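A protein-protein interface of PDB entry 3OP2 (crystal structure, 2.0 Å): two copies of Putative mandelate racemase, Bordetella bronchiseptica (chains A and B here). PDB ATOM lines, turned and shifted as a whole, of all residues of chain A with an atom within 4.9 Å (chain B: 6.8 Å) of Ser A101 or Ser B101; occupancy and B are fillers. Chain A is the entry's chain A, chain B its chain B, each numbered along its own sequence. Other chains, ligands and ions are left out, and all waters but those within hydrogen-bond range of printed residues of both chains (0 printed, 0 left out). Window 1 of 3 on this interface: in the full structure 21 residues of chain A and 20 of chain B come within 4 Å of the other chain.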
ATOM      1  N   SER A 101       6.585 -10.682 -24.678  1.00  0.00           N
ATOM      2  CA  SER A 101       5.446 -10.041 -24.036  1.00  0.00           C
ATOM      3  C   SER A 101       5.566 -10.181 -22.523  1.00  0.00           C
ATOM      4  O   SER A 101       6.633 -10.526 -22.012  1.00  0.00           O
ATOM      5  CB  SER A 101       4.143 -10.667 -24.542  1.00  0.00           C
ATOM      6  OG  SER A 101       4.158 -12.073 -24.401  1.00  0.00           O
ATOM      7  N   VAL A 102       4.477  -9.896 -21.810  1.00  0.00           N
ATOM      8  CA  VAL A 102       4.390 -10.177 -20.374  1.00  0.00           C
ATOM      9  C   VAL A 102       4.018 -11.656 -20.156  1.00  0.00           C
ATOM     10  O   VAL A 102       4.149 -12.188 -19.047  1.00  0.00           O
ATOM     11  CB  VAL A 102       3.374  -9.241 -19.666  1.00  0.00           C
ATOM     12  CG1 VAL A 102       1.978  -9.871 -19.632  1.00  0.00           C
ATOM     13  CG2 VAL A 102       3.857  -8.890 -18.258  1.00  0.00           C
ATOM     14  N   GLY A 103       3.548 -12.298 -21.230  1.00  0.00           N
ATOM     15  CA  GLY A 103       3.275 -13.731 -21.248  1.00  0.00           C
ATOM     16  C   GLY A 103       4.568 -14.522 -21.339  1.00  0.00           C
ATOM     17  O   GLY A 103       4.765 -15.476 -20.583  1.00  0.00           O
ATOM     18  N   ILE A 104       5.436 -14.119 -22.273  1.00  0.00           N
ATOM     19  CA  ILE A 104       6.792 -14.663 -22.388  1.00  0.00           C
ATOM     20  C   ILE A 104       7.599 -14.324 -21.132  1.00  0.00           C
ATOM     21  O   ILE A 104       8.389 -15.141 -20.672  1.00  0.00           O
ATOM     22  CB  ILE A 104       7.564 -14.135 -23.636  1.00  0.00           C
ATOM     23  CG1 ILE A 104       6.729 -14.218 -24.931  1.00  0.00           C
ATOM     24  CG2 ILE A 104       8.899 -14.863 -23.801  1.00  0.00           C
ATOM     25  CD1 ILE A 104       5.976 -15.526 -25.153  1.00  0.00           C
ATOM     26  N   ALA A 105       7.412 -13.117 -20.599  1.00  0.00           N
ATOM     27  CA  ALA A 105       8.087 -12.716 -19.359  1.00  0.00           C
ATOM     28  C   ALA A 105       7.707 -13.656 -18.216  1.00  0.00           C
ATOM     29  O   ALA A 105       8.577 -14.191 -17.519  1.00  0.00           O
ATOM     30  CB  ALA A 105       7.751 -11.260 -19.000  1.00  0.00           C
ATOM     31  N   TYR A 257      11.553 -10.316 -27.287  1.00  0.00           N
ATOM     32  CA  TYR A 257      11.157 -11.405 -26.400  1.00  0.00           C
ATOM     33  C   TYR A 257      11.060 -12.777 -27.080  1.00  0.00           C
ATOM     34  O   TYR A 257      10.832 -13.791 -26.410  1.00  0.00           O
ATOM     35  CB  TYR A 257       9.851 -11.038 -25.671  1.00  0.00           C
ATOM     36  CG  TYR A 257       9.917  -9.700 -24.953  1.00  0.00           C
ATOM     37  CD1 TYR A 257       9.407  -8.547 -25.538  1.00  0.00           C
ATOM     38  CD2 TYR A 257      10.510  -9.583 -23.695  1.00  0.00           C
ATOM     39  CE1 TYR A 257       9.475  -7.308 -24.886  1.00  0.00           C
ATOM     40  CE2 TYR A 257      10.590  -8.337 -23.034  1.00  0.00           C
ATOM     41  CZ  TYR A 257      10.066  -7.211 -23.639  1.00  0.00           C
ATOM     42  OH  TYR A 257      10.127  -5.983 -23.006  1.00  0.00           O
ATOM     43  N   TYR B  56      -8.091 -14.096 -23.388  1.00  0.00           N
ATOM     44  CA  TYR B  56      -6.865 -13.841 -22.629  1.00  0.00           C
ATOM     45  C   TYR B  56      -7.313 -13.785 -21.178  1.00  0.00           C
ATOM     46  O   TYR B  56      -8.497 -13.603 -20.926  1.00  0.00           O
ATOM     47  CB  TYR B  56      -6.258 -12.485 -23.014  1.00  0.00           C
ATOM     48  CG  TYR B  56      -6.063 -12.258 -24.504  1.00  0.00           C
ATOM     49  CD1 TYR B  56      -5.141 -13.017 -25.229  1.00  0.00           C
ATOM     50  CD2 TYR B  56      -6.779 -11.270 -25.182  1.00  0.00           C
ATOM     51  CE1 TYR B  56      -4.949 -12.816 -26.597  1.00  0.00           C
ATOM     52  CE2 TYR B  56      -6.595 -11.052 -26.559  1.00  0.00           C
ATOM     53  CZ  TYR B  56      -5.671 -11.834 -27.259  1.00  0.00           C
ATOM     54  OH  TYR B  56      -5.468 -11.648 -28.616  1.00  0.00           O
ATOM     55  N   VAL B  93       3.793   0.417 -21.253  1.00  0.00           N
ATOM     56  CA  VAL B  93       3.540  -0.974 -21.707  1.00  0.00           C
ATOM     57  C   VAL B  93       4.739  -1.638 -22.418  1.00  0.00           C
ATOM     58  O   VAL B  93       4.890  -2.869 -22.372  1.00  0.00           O
ATOM     59  CB  VAL B  93       2.215  -1.114 -22.551  1.00  0.00           C
ATOM     60  CG1 VAL B  93       2.239  -2.358 -23.469  1.00  0.00           C
ATOM     61  CG2 VAL B  93       0.991  -1.161 -21.638  1.00  0.00           C
ATOM     62  N   SER B 101       0.948  -9.516 -28.142  1.00  0.00           N
ATOM     63  CA  SER B 101       1.001  -9.476 -26.685  1.00  0.00           C
ATOM     64  C   SER B 101      -0.338  -9.048 -26.068  1.00  0.00           C
ATOM     65  O   SER B 101      -1.180  -8.444 -26.720  1.00  0.00           O
ATOM     66  CB  SER B 101       2.147  -8.565 -26.204  1.00  0.00           C
ATOM     67  OG  SER B 101       1.772  -7.200 -26.171  1.00  0.00           O
ATOM     68  N   VAL B 102      -0.515  -9.375 -24.794  1.00  0.00           N
ATOM     69  CA  VAL B 102      -1.703  -8.973 -24.048  1.00  0.00           C
ATOM     70  C   VAL B 102      -1.715  -7.448 -23.810  1.00  0.00           C
ATOM     71  O   VAL B 102      -2.759  -6.868 -23.535  1.00  0.00           O
ATOM     72  CB  VAL B 102      -1.811  -9.770 -22.708  1.00  0.00           C
ATOM     73  CG1 VAL B 102      -0.867  -9.199 -21.650  1.00  0.00           C
ATOM     74  CG2 VAL B 102      -3.251  -9.810 -22.200  1.00  0.00           C
ATOM     75  N   GLY B 103      -0.546  -6.818 -23.931  1.00  0.00           N
ATOM     76  CA  GLY B 103      -0.403  -5.371 -23.744  1.00  0.00           C
ATOM     77  C   GLY B 103      -0.957  -4.593 -24.926  1.00  0.00           C
ATOM     78  O   GLY B 103      -1.696  -3.624 -24.746  1.00  0.00           O
ATOM     79  N   ILE B 104      -0.584  -5.021 -26.132  1.00  0.00           N
ATOM     80  CA  ILE B 104      -1.120  -4.452 -27.365  1.00  0.00           C
ATOM     81  C   ILE B 104      -2.626  -4.704 -27.415  1.00  0.00           C
ATOM     82  O   ILE B 104      -3.377  -3.866 -27.887  1.00  0.00           O
ATOM     83  CB  ILE B 104      -0.450  -5.055 -28.644  1.00  0.00           C
ATOM     84  CG1 ILE B 104       1.085  -4.967 -28.590  1.00  0.00           C
ATOM     85  CG2 ILE B 104      -0.999  -4.400 -29.926  1.00  0.00           C
ATOM     86  CD1 ILE B 104       1.656  -3.546 -28.642  1.00  0.00           C
ATOM     87  N   ALA B 105      -3.051  -5.868 -26.929  1.00  0.00           N
ATOM     88  CA  ALA B 105      -4.475  -6.204 -26.862  1.00  0.00           C
ATOM     89  C   ALA B 105      -5.199  -5.208 -25.958  1.00  0.00           C
ATOM     90  O   ALA B 105      -6.212  -4.617 -26.343  1.00  0.00           O
ATOM     91  CB  ALA B 105      -4.664  -7.645 -26.354  1.00  0.00           C
ATOM     92  N   ALA B 106      -4.644  -5.006 -24.763  1.00  0.00           N
ATOM     93  CA  ALA B 106      -5.192  -4.076 -23.782  1.00  0.00           C
ATOM     94  C   ALA B 106      -5.328  -2.674 -24.369  1.00  0.00           C
ATOM     95  O   ALA B 106      -6.380  -2.047 -24.244  1.00  0.00           O
ATOM     96  CB  ALA B 106      -4.319  -4.068 -22.522  1.00  0.00           C
ATOM     97  N   ASN B 255      -3.199 -13.753 -34.937  1.00  0.00           N
ATOM     98  CA  ASN B 255      -2.244 -13.916 -33.854  1.00  0.00           C
ATOM     99  C   ASN B 255      -0.986 -13.075 -34.072  1.00  0.00           C
ATOM    100  O   ASN B 255       0.020 -13.284 -33.401  1.00  0.00           O
ATOM    101  CB  ASN B 255      -1.902 -15.407 -33.681  1.00  0.00           C
ATOM    102  CG  ASN B 255      -3.068 -16.207 -33.109  1.00  0.00           C
ATOM    103  OD1 ASN B 255      -3.708 -15.789 -32.139  1.00  0.00           O
ATOM    104  ND2 ASN B 255      -3.350 -17.350 -33.703  1.00  0.00           N
ATOM    105  N   LEU B 256      -1.046 -12.133 -35.016  1.00  0.00           N
ATOM    106  CA  LEU B 256       0.027 -11.153 -35.203  1.00  0.00           C
ATOM    107  C   LEU B 256      -0.403  -9.832 -34.570  1.00  0.00           C
ATOM    108  O   LEU B 256      -1.567  -9.441 -34.681  1.00  0.00           O
ATOM    109  CB  LEU B 256       0.370 -10.974 -36.685  1.00  0.00           C
ATOM    110  CG  LEU B 256       0.883 -12.191 -37.484  1.00  0.00           C
ATOM    111  CD1 LEU B 256       1.085 -11.819 -38.941  1.00  0.00           C
ATOM    112  CD2 LEU B 256       2.160 -12.767 -36.889  1.00  0.00           C
ATOM    113  N   TYR B 257       0.530  -9.151 -33.911  1.00  0.00           N
ATOM    114  CA  TYR B 257       0.168  -8.025 -33.051  1.00  0.00           C
ATOM    115  C   TYR B 257       0.764  -6.652 -33.432  1.00  0.00           C
ATOM    116  O   TYR B 257       0.462  -5.642 -32.783  1.00  0.00           O
ATOM    117  CB  TYR B 257       0.436  -8.380 -31.577  1.00  0.00           C
ATOM    118  CG  TYR B 257      -0.543  -9.405 -31.026  1.00  0.00           C
ATOM    119  CD1 TYR B 257      -0.310 -10.772 -31.172  1.00  0.00           C
ATOM    120  CD2 TYR B 257      -1.708  -9.007 -30.369  1.00  0.00           C
ATOM    121  CE1 TYR B 257      -1.217 -11.721 -30.683  1.00  0.00           C
ATOM    122  CE2 TYR B 257      -2.619  -9.946 -29.869  1.00  0.00           C
ATOM    123  CZ  TYR B 257      -2.365 -11.302 -30.038  1.00  0.00           C
ATOM    124  OH  TYR B 257      -3.250 -12.233 -29.553  1.00  0.00           O
ATOM    125  N   ARG B 280      -7.082  -6.488 -31.523  1.00  0.00           N
ATOM    126  CA  ARG B 280      -5.877  -7.194 -31.083  1.00  0.00           C
ATOM    127  C   ARG B 280      -4.590  -6.486 -31.487  1.00  0.00           C
ATOM    128  O   ARG B 280      -3.594  -6.526 -30.769  1.00  0.00           O
ATOM    129  CB  ARG B 280      -5.877  -8.637 -31.625  1.00  0.00           C
ATOM    130  CG  ARG B 280      -6.682  -9.600 -30.759  1.00  0.00           C
ATOM    131  CD  ARG B 280      -7.523 -10.607 -31.548  1.00  0.00           C
ATOM    132  NE  ARG B 280      -6.811 -11.805 -31.952  1.00  0.00           N
ATOM    133  CZ  ARG B 280      -7.168 -13.064 -31.675  1.00  0.00           C
ATOM    134  NH1 ARG B 280      -8.244 -13.358 -30.958  1.00  0.00           N
ATOM    135  NH2 ARG B 280      -6.414 -14.040 -32.134  1.00  0.00           N
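Ser A101 touches Ser B101 (CB to CB, 3.3 Å). Val B102 touches Val A102 (CG1 to CG1, 3.6 Å).
N of Ile B104 sits at hydrogen-bond distance from OG of Ser B101 (3.2 Å). OG of Ser A101 lies within hydrogen-bond range of N of Ile A104 (3.2 Å). The side-chain hydroxyl (OG) of Ser B101 sits close to the backbone NH (N) of Gly B103, at 3.2 Å. The side-chain hydroxyl of Ser A101 lies close to the backbone NH of Gly A103, at 3.2 Å.
Ser B101 touches its own counterpart, Ser A101. Val A102 touches its own counterpart, Val B102.
Of the 6 printed residues of chain A, 2 touch a printed residue of chain B. Hydrophobic or aromatic side chains of chain A within 4 Å of the printed part of chain B: Val A102. Printed residues of chain B that touch a printed residue of chain A: Ser B101 and Val B102. Hydrophobic or aromatic side chains of chain B that line the printed part of chain A: Val B102. Among the printed residues, 2 pairs touch across the chains. Among the printed residues, no Asp or Glu carboxylate lies within 4 Å of a Lys or Arg side-chain nitrogen of the other chain.
Of chain B, only Ser B101 comes within 4 Å of Ser A101. Printed residues of chain B within 4 Å of Val A102: Val B102. Ser B101 touches just one residue of chain A: Ser A101. Of the printed residues of chain A, Val B102 touches Val A102. The nearest printed residue of chain A that does not touch Val B102 is Ser A101 (4.8 Å).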
